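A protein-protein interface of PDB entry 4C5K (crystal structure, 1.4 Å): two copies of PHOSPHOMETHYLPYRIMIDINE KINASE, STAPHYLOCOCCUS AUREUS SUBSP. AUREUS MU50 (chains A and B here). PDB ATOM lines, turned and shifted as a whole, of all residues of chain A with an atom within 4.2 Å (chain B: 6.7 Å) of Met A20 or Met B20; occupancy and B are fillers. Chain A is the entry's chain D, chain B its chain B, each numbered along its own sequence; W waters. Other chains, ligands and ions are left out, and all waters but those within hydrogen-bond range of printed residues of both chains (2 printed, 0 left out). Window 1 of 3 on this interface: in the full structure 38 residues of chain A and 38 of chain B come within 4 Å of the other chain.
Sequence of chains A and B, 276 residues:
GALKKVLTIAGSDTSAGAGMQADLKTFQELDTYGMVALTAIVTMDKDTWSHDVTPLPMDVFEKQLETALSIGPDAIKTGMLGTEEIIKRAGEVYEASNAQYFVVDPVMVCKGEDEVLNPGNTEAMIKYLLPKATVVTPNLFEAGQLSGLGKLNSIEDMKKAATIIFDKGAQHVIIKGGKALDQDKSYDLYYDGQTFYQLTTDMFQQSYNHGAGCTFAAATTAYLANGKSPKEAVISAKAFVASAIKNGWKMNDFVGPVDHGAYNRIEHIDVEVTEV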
ATOM      1  N   ALA A  10      26.237 -10.086   9.896  1.00  0.00           N
ATOM      2  CA  ALA A  10      26.341 -11.498  10.025  1.00  0.00           C
ATOM      3  C   ALA A  10      25.538 -12.231   8.947  1.00  0.00           C
ATOM      4  O   ALA A  10      24.663 -11.627   8.310  1.00  0.00           O
ATOM      5  CB  ALA A  10      25.802 -11.919  11.402  1.00  0.00           C
ATOM      6  N   GLY A  11      25.734 -13.517   8.855  1.00  0.00           N
ATOM      7  CA  GLY A  11      25.005 -14.387   7.962  1.00  0.00           C
ATOM      8  C   GLY A  11      23.802 -15.046   8.625  1.00  0.00           C
ATOM      9  O   GLY A  11      23.699 -15.076   9.869  1.00  0.00           O
ATOM     10  N   SER A  12      22.929 -15.602   7.817  1.00  0.00           N
ATOM     11  CA  SER A  12      21.811 -16.366   8.278  1.00  0.00           C
ATOM     12  C   SER A  12      22.212 -17.822   8.496  1.00  0.00           C
ATOM     13  O   SER A  12      22.680 -18.492   7.584  1.00  0.00           O
ATOM     14  CB  SER A  12      20.656 -16.307   7.274  1.00  0.00           C
ATOM     15  OG  SER A  12      19.565 -17.053   7.743  1.00  0.00           O
ATOM     16  N   ALA A  18      22.682 -20.092  15.719  1.00  0.00           N
ATOM     17  CA  ALA A  18      23.847 -19.198  15.607  1.00  0.00           C
ATOM     18  C   ALA A  18      23.563 -18.102  14.621  1.00  0.00           C
ATOM     19  O   ALA A  18      22.418 -17.796  14.334  1.00  0.00           O
ATOM     20  CB  ALA A  18      25.105 -20.020  15.290  1.00  0.00           C
ATOM     21  N   GLY A  19      24.597 -17.445  14.097  1.00  0.00           N
ATOM     22  CA  GLY A  19      24.413 -16.448  13.090  1.00  0.00           C
ATOM     23  C   GLY A  19      23.580 -15.298  13.578  1.00  0.00           C
ATOM     24  O   GLY A  19      23.432 -14.985  14.762  1.00  0.00           O
ATOM     25  N   MET A  20      22.955 -14.618  12.618  1.00  0.00           N
ATOM     26  CA  MET A  20      22.125 -13.463  12.886  1.00  0.00           C
ATOM     27  C   MET A  20      20.910 -13.843  13.729  1.00  0.00           C
ATOM     28  O   MET A  20      20.396 -12.993  14.441  1.00  0.00           O
ATOM     29  CB  MET A  20      21.733 -12.711  11.606  1.00  0.00           C
ATOM     30  CG  MET A  20      20.814 -13.500  10.704  1.00  0.00           C
ATOM     31  SD  MET A  20      19.062 -13.104  11.042  1.00  0.00           S
ATOM     32  CE  MET A  20      18.291 -14.068   9.744  1.00  0.00           C
ATOM     33  N   GLN A  21      20.470 -15.099  13.616  1.00  0.00           N
ATOM     34  CA  GLN A  21      19.330 -15.551  14.390  1.00  0.00           C
ATOM     35  C   GLN A  21      19.659 -15.490  15.909  1.00  0.00           C
ATOM     36  O   GLN A  21      18.912 -14.924  16.678  1.00  0.00           O
ATOM     37  CB  GLN A  21      18.960 -16.952  14.006  1.00  0.00           C
ATOM     38  CG  GLN A  21      18.186 -17.046  12.666  1.00  0.00           C
ATOM     39  CD  GLN A  21      19.060 -17.152  11.438  1.00  0.00           C
ATOM     40  OE1 GLN A  21      20.232 -16.820  11.451  1.00  0.00           O
ATOM     41  NE2 GLN A  21      18.477 -17.599  10.343  1.00  0.00           N
ATOM     42  N   ALA A  22      20.852 -16.016  16.270  1.00  0.00           N
ATOM     43  CA  ALA A  22      21.243 -15.922  17.697  1.00  0.00           C
ATOM     44  C   ALA A  22      21.332 -14.460  18.105  1.00  0.00           C
ATOM     45  O   ALA A  22      20.959 -14.083  19.214  1.00  0.00           O
ATOM     46  CB  ALA A  22      22.621 -16.576  17.898  1.00  0.00           C
ATOM     47  N   ASP A  23      21.894 -13.627  17.214  1.00  0.00           N
ATOM     48  CA  ASP A  23      22.047 -12.211  17.498  1.00  0.00           C
ATOM     49  C   ASP A  23      20.714 -11.501  17.786  1.00  0.00           C
ATOM     50  O   ASP A  23      20.513 -10.900  18.834  1.00  0.00           O
ATOM     51  CB  ASP A  23      22.828 -11.514  16.408  1.00  0.00           C
ATOM     52  CG  ASP A  23      24.251 -12.026  16.207  1.00  0.00           C
ATOM     53  OD1 ASP A  23      24.816 -12.599  17.164  1.00  0.00           O
ATOM     54  OD2 ASP A  23      24.771 -11.889  15.069  1.00  0.00           O
ATOM     55  N   LEU A  24      19.791 -11.624  16.834  1.00  0.00           N
ATOM     56  CA  LEU A  24      18.509 -11.006  17.005  1.00  0.00           C
ATOM     57  C   LEU A  24      17.731 -11.525  18.200  1.00  0.00           C
ATOM     58  O   LEU A  24      17.086 -10.747  18.897  1.00  0.00           O
ATOM     59  CB  LEU A  24      17.642 -11.150  15.749  1.00  0.00           C
ATOM     60  CG  LEU A  24      18.135 -10.443  14.487  1.00  0.00           C
ATOM     61  CD1 LEU A  24      17.155 -10.712  13.387  1.00  0.00           C
ATOM     62  CD2 LEU A  24      18.370  -8.927  14.713  1.00  0.00           C
ATOM     63  N   VAL A  36      19.799  -6.340  11.530  1.00  0.00           N
ATOM     64  CA  VAL A  36      20.785  -7.156  10.850  1.00  0.00           C
ATOM     65  C   VAL A  36      21.076  -6.623   9.440  1.00  0.00           C
ATOM     66  O   VAL A  36      20.160  -6.258   8.694  1.00  0.00           O
ATOM     67  CB  VAL A  36      20.381  -8.648  10.780  1.00  0.00           C
ATOM     68  CG1 VAL A  36      19.032  -8.887  10.171  1.00  0.00           C
ATOM     69  CG2 VAL A  36      21.427  -9.458   9.996  1.00  0.00           C
ATOM     70  N   LEU A  38      22.616  -8.627   6.459  1.00  0.00           N
ATOM     71  CA  LEU A  38      22.907 -10.004   6.084  1.00  0.00           C
ATOM     72  C   LEU A  38      24.044 -10.104   5.052  1.00  0.00           C
ATOM     73  O   LEU A  38      24.001  -9.436   4.005  1.00  0.00           O
ATOM     74  CB  LEU A  38      21.662 -10.685   5.497  1.00  0.00           C
ATOM     75  CG  LEU A  38      20.462 -10.768   6.413  1.00  0.00           C
ATOM     76  CD1 LEU A  38      19.233 -11.032   5.582  1.00  0.00           C
ATOM     77  CD2 LEU A  38      20.709 -11.875   7.418  1.00  0.00           C
ATOM     78  N   THR B   8       8.933 -19.150   9.967  1.00  0.00           N
ATOM     79  CA  THR B   8       8.324 -18.160   9.105  1.00  0.00           C
ATOM     80  C   THR B   8       8.959 -18.264   7.731  1.00  0.00           C
ATOM     81  O   THR B   8      10.195 -18.444   7.583  1.00  0.00           O
ATOM     82  CB  THR B   8       8.409 -16.722   9.640  1.00  0.00           C
ATOM     83  OG1 THR B   8       7.627 -15.890   8.773  1.00  0.00           O
ATOM     84  CG2 THR B   8       9.837 -16.253   9.784  1.00  0.00           C
ATOM     85  N   ILE B   9       8.126 -18.129   6.697  1.00  0.00           N
ATOM     86  CA  ILE B   9       8.535 -17.999   5.299  1.00  0.00           C
ATOM     87  C   ILE B   9       8.275 -16.562   4.914  1.00  0.00           C
ATOM     88  O   ILE B   9       7.121 -16.123   4.800  1.00  0.00           O
ATOM     89  CB  ILE B   9       7.827 -18.990   4.398  1.00  0.00           C
ATOM     90  CG1 ILE B   9       8.005 -20.448   4.908  1.00  0.00           C
ATOM     91  CG2 ILE B   9       8.248 -18.791   2.954  1.00  0.00           C
ATOM     92  CD1 ILE B   9       7.131 -21.477   4.198  1.00  0.00           C
ATOM     93  N   ALA B  10       9.314 -15.762   4.809  1.00  0.00           N
ATOM     94  CA  ALA B  10       9.236 -14.334   4.798  1.00  0.00           C
ATOM     95  C   ALA B  10      10.503 -13.654   4.302  1.00  0.00           C
ATOM     96  O   ALA B  10      11.557 -14.281   4.268  1.00  0.00           O
ATOM     97  CB  ALA B  10       8.820 -13.755   6.135  1.00  0.00           C
ATOM     98  N   GLY B  11      10.390 -12.387   3.974  1.00  0.00           N
ATOM     99  CA  GLY B  11      11.501 -11.557   3.604  1.00  0.00           C
ATOM    100  C   GLY B  11      12.097 -10.784   4.744  1.00  0.00           C
ATOM    101  O   GLY B  11      11.488 -10.607   5.808  1.00  0.00           O
ATOM    102  N   SER B  12      13.287 -10.264   4.502  1.00  0.00           N
ATOM    103  CA  SER B  12      13.978  -9.392   5.439  1.00  0.00           C
ATOM    104  C   SER B  12      13.568  -7.946   5.273  1.00  0.00           C
ATOM    105  O   SER B  12      13.726  -7.387   4.191  1.00  0.00           O
ATOM    106  CB  SER B  12      15.477  -9.539   5.339  1.00  0.00           C
ATOM    107  OG  SER B  12      16.164  -8.737   6.268  1.00  0.00           O
ATOM    108  N   ASP B  13      13.054  -7.352   6.354  1.00  0.00           N
ATOM    109  CA  ASP B  13      12.819  -5.903   6.425  1.00  0.00           C
ATOM    110  C   ASP B  13      14.039  -5.279   7.042  1.00  0.00           C
ATOM    111  O   ASP B  13      14.201  -5.414   8.248  1.00  0.00           O
ATOM    112  CB  ASP B  13      11.588  -5.625   7.324  1.00  0.00           C
ATOM    113  CG  ASP B  13      11.443  -4.150   7.715  1.00  0.00           C
ATOM    114  OD1 ASP B  13      12.099  -3.273   7.087  1.00  0.00           O
ATOM    115  OD2 ASP B  13      10.695  -3.861   8.699  1.00  0.00           O
ATOM    116  N   ALA B  18       9.255  -5.066  10.755  1.00  0.00           N
ATOM    117  CA  ALA B  18       8.319  -5.960  10.104  1.00  0.00           C
ATOM    118  C   ALA B  18       9.075  -7.129   9.548  1.00  0.00           C
ATOM    119  O   ALA B  18      10.220  -7.420   9.963  1.00  0.00           O
ATOM    120  CB  ALA B  18       7.504  -5.206   9.049  1.00  0.00           C
ATOM    121  N   GLY B  19       8.480  -7.858   8.633  1.00  0.00           N
ATOM    122  CA  GLY B  19       9.152  -8.943   7.963  1.00  0.00           C
ATOM    123  C   GLY B  19       9.555 -10.078   8.893  1.00  0.00           C
ATOM    124  O   GLY B  19       9.017 -10.246  10.011  1.00  0.00           O
ATOM    125  N   MET B  20      10.628 -10.779   8.517  1.00  0.00           N
ATOM    126  CA  MET B  20      11.103 -11.908   9.303  1.00  0.00           C
ATOM    127  C   MET B  20      11.626 -11.415  10.641  1.00  0.00           C
ATOM    128  O   MET B  20      11.628 -12.169  11.607  1.00  0.00           O
ATOM    129  CB  MET B  20      12.126 -12.710   8.529  1.00  0.00           C
ATOM    130  CG  MET B  20      13.414 -12.025   8.274  1.00  0.00           C
ATOM    131  SD  MET B  20      14.658 -12.337   9.556  1.00  0.00           S
ATOM    132  CE  MET B  20      16.065 -11.494   8.864  1.00  0.00           C
ATOM    133  N   GLN B  21      12.087 -10.179  10.695  1.00  0.00           N
ATOM    134  CA  GLN B  21      12.584  -9.613  11.941  1.00  0.00           C
ATOM    135  C   GLN B  21      11.466  -9.543  12.999  1.00  0.00           C
ATOM    136  O   GLN B  21      11.623 -10.005  14.141  1.00  0.00           O
ATOM    137  CB  GLN B  21      13.187  -8.233  11.720  1.00  0.00           C
ATOM    138  CG  GLN B  21      14.531  -8.185  11.085  1.00  0.00           C
ATOM    139  CD  GLN B  21      14.499  -8.218   9.544  1.00  0.00           C
ATOM    140  OE1 GLN B  21      13.539  -8.643   8.903  1.00  0.00           O
ATOM    141  NE2 GLN B  21      15.664  -7.892   8.951  1.00  0.00           N
ATOM    142  N   ALA B  22      10.321  -8.986  12.599  1.00  0.00           N
ATOM    143  CA  ALA B  22       9.203  -8.987  13.519  1.00  0.00           C
ATOM    144  C   ALA B  22       8.822 -10.424  13.924  1.00  0.00           C
ATOM    145  O   ALA B  22       8.475 -10.666  15.095  1.00  0.00           O
ATOM    146  CB  ALA B  22       7.999  -8.310  12.882  1.00  0.00           C
ATOM    147  N   ASP B  23       8.845 -11.348  12.971  1.00  0.00           N
ATOM    148  CA  ASP B  23       8.478 -12.712  13.240  1.00  0.00           C
ATOM    149  C   ASP B  23       9.434 -13.339  14.277  1.00  0.00           C
ATOM    150  O   ASP B  23       8.981 -13.884  15.281  1.00  0.00           O
ATOM    151  CB  ASP B  23       8.469 -13.542  11.975  1.00  0.00           C
ATOM    152  CG  ASP B  23       7.462 -13.067  10.926  1.00  0.00           C
ATOM    153  OD1 ASP B  23       6.455 -12.433  11.333  1.00  0.00           O
ATOM    154  OD2 ASP B  23       7.651 -13.385   9.722  1.00  0.00           O
ATOM    155  N   LEU B  24      10.752 -13.276  14.023  1.00  0.00           N
ATOM    156  CA  LEU B  24      11.697 -13.887  14.938  1.00  0.00           C
ATOM    157  C   LEU B  24      11.593 -13.227  16.324  1.00  0.00           C
ATOM    158  O   LEU B  24      11.730 -13.907  17.361  1.00  0.00           O
ATOM    159  CB  LEU B  24      13.122 -13.823  14.401  1.00  0.00           C
ATOM    160  CG  LEU B  24      13.418 -14.641  13.178  1.00  0.00           C
ATOM    161  CD1 LEU B  24      14.881 -14.448  12.794  1.00  0.00           C
ATOM    162  CD2 LEU B  24      13.124 -16.106  13.373  1.00  0.00           C
ATOM    163  N   LYS B  25      11.465 -11.904  16.361  1.00  0.00           N
ATOM    164  CA  LYS B  25      11.390 -11.191  17.629  1.00  0.00           C
ATOM    165  C   LYS B  25      10.161 -11.653  18.420  1.00  0.00           C
ATOM    166  O   LYS B  25      10.212 -11.852  19.651  1.00  0.00           O
ATOM    167  CB  LYS B  25      11.382  -9.682  17.402  1.00  0.00           C
ATOM    168  CG  LYS B  25      12.664  -9.124  16.854  1.00  0.00           C
ATOM    169  CD  LYS B  25      12.591  -7.675  16.422  1.00  0.00           C
ATOM    170  CE  LYS B  25      13.892  -7.126  15.900  1.00  0.00           C
ATOM    171  NZ  LYS B  25      13.956  -5.692  15.764  1.00  0.00           N
ATOM    172  N   THR B  26       9.036 -11.764  17.746  1.00  0.00           N
ATOM    173  CA  THR B  26       7.779 -12.158  18.363  1.00  0.00           C
ATOM    174  C   THR B  26       7.798 -13.601  18.799  1.00  0.00           C
ATOM    175  O   THR B  26       7.384 -13.934  19.919  1.00  0.00           O
ATOM    176  CB  THR B  26       6.605 -11.867  17.377  1.00  0.00           C
ATOM    177  OG1 THR B  26       6.550 -10.473  17.087  1.00  0.00           O
ATOM    178  CG2 THR B  26       5.283 -12.309  17.933  1.00  0.00           C
ATOM    179  N   PHE B  27       8.313 -14.487  17.957  1.00  0.00           N
ATOM    180  CA  PHE B  27       8.503 -15.877  18.343  1.00  0.00           C
ATOM    181  C   PHE B  27       9.328 -16.011  19.640  1.00  0.00           C
ATOM    182  O   PHE B  27       9.047 -16.826  20.493  1.00  0.00           O
ATOM    183  CB  PHE B  27       9.165 -16.683  17.233  1.00  0.00           C
ATOM    184  CG  PHE B  27       8.371 -16.774  15.950  1.00  0.00           C
ATOM    185  CD1 PHE B  27       6.992 -16.585  15.877  1.00  0.00           C
ATOM    186  CD2 PHE B  27       9.027 -17.085  14.783  1.00  0.00           C
ATOM    187  CE1 PHE B  27       6.324 -16.675  14.677  1.00  0.00           C
ATOM    188  CE2 PHE B  27       8.373 -17.213  13.562  1.00  0.00           C
ATOM    189  CZ  PHE B  27       7.001 -17.003  13.516  1.00  0.00           C
ATOM    190  N   VAL B  36      13.579 -19.038  10.190  1.00  0.00           N
ATOM    191  CA  VAL B  36      13.166 -18.344   8.978  1.00  0.00           C
ATOM    192  C   VAL B  36      13.705 -19.031   7.720  1.00  0.00           C
ATOM    193  O   VAL B  36      14.881 -19.451   7.655  1.00  0.00           O
ATOM    194  CB  VAL B  36      13.554 -16.857   9.002  1.00  0.00           C
ATOM    195  CG1 VAL B  36      15.058 -16.600   9.265  1.00  0.00           C
ATOM    196  CG2 VAL B  36      13.132 -16.125   7.730  1.00  0.00           C
ATOM    197  N   ALA B  37      12.862 -19.094   6.678  1.00  0.00           N
ATOM    198  CA  ALA B  37      13.305 -19.382   5.309  1.00  0.00           C
ATOM    199  C   ALA B  37      13.094 -18.065   4.547  1.00  0.00           C
ATOM    200  O   ALA B  37      11.944 -17.643   4.337  1.00  0.00           O
ATOM    201  CB  ALA B  37      12.542 -20.537   4.681  1.00  0.00           C
ATOM    202  N   LEU B  38      14.190 -17.399   4.205  1.00  0.00           N
ATOM    203  CA  LEU B  38      14.198 -16.091   3.590  1.00  0.00           C
ATOM    204  C   LEU B  38      13.831 -16.155   2.111  1.00  0.00           C
ATOM    205  O   LEU B  38      14.401 -16.939   1.346  1.00  0.00           O
ATOM    206  CB  LEU B  38      15.560 -15.442   3.716  1.00  0.00           C
ATOM    207  CG  LEU B  38      16.012 -15.165   5.139  1.00  0.00           C
ATOM    208  CD1 LEU B  38      17.502 -14.970   5.208  1.00  0.00           C
ATOM    209  CD2 LEU B  38      15.313 -13.934   5.708  1.00  0.00           C
ATOM    210  N   ALA B  40      13.456 -12.931   0.224  1.00  0.00           N
ATOM    211  CA  ALA B  40      13.747 -11.647  -0.331  1.00  0.00           C
ATOM    212  C   ALA B  40      14.398 -10.774   0.717  1.00  0.00           C
ATOM    213  O   ALA B  40      14.274 -11.047   1.903  1.00  0.00           O
ATOM    214  CB  ALA B  40      12.497 -10.954  -0.848  1.00  0.00           C
ATOM    215  N   CYS B 214       2.588  -7.928  10.773  1.00  0.00           N
ATOM    216  CA  CYS B 214       3.450  -9.077  10.859  1.00  0.00           C
ATOM    217  C   CYS B 214       3.479  -9.652  12.262  1.00  0.00           C
ATOM    218  O   CYS B 214       3.412 -10.849  12.444  1.00  0.00           O
ATOM    219  CB  CYS B 214       4.863  -8.689  10.406  1.00  0.00           C
ATOM    220  SG  CYS B 214       5.060  -8.373   8.646  1.00  0.00           S
HETATM  221  O   HOH W   1      16.336 -19.713   9.996  1.00  0.00           O
HETATM  222  O   HOH W   2      17.671  -5.758   9.683  1.00  0.00           O
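Ser A12 touches Leu B38, and with the chains exchanged Leu A38 touches Ser B12. Met A20 touches its own counterpart, Met B20. Gln A21 touches Val B36, and with the chains exchanged Val A36 touches Gln B21. 12 positions are printed for both chains. Of the 5 pairs that touch across the chains among the printed residues, 5 have their exchanged pair printed and touching as well.
Along chain A the printed residues that touch a printed residue of chain B span positions 12 to 38. Among the printed residues, 5 pairs touch across the chains. Among the printed residues, no Asp or Glu carboxylate lies within 4 Å of a Lys or Arg side-chain nitrogen of the other chain.
Of the printed residues of chain B, Ser A12 touches Leu B38. Gly A19 touches none of the printed residues of chain B. Met A20 touches one residue of chain B. Of the printed residues of chain B, Gln A21 touches Val B36. Thr B26 touches none of the printed residues of chain A. The nearest printed residue of chain A that does not touch Met B20 is Val A36 (4.2 Å).
O of Gly B11 lies within hydrogen-bond range of N of Met B20 (2.8 Å). OG of Ser B12 is in hydrogen-bond range of NE2 of Gln B21. The backbone NH of Ser B12 lies within hydrogen-bond range of the backbone carbonyl oxygen of Ala B40 (2.9 Å). N of Asp B13 sits at hydrogen-bond distance from OE1 of Gln B21 (2.9 Å). The backbone carbonyl oxygen (O) of Gly A11 is in hydrogen-bond range of the backbone NH (N) of Met A20, 2.9 Å away. The side-chain hydroxyl of Ser A12 lies within hydrogen-bond range of the side-chain amide nitrogen of Gln A21 (2.9 Å).
Leu B38 touches Ser A12. CE of Met A20 touches CE of Met B20 (3.5 Å). CG1 of Val B36 touches NE2 of Gln A21, 3.7 Å away. Gln B21 touches Val A36. Leu A38 touches Ser B12.
Water W2 bridges the backbone carbonyl oxygen (O) of Val A36 and the side-chain amide nitrogen (NE2) of Gln B21. Water W1 bridges the backbone carbonyl oxygen (O) of Val B36 and the side-chain amide nitrogen (NE2) of Gln A21.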
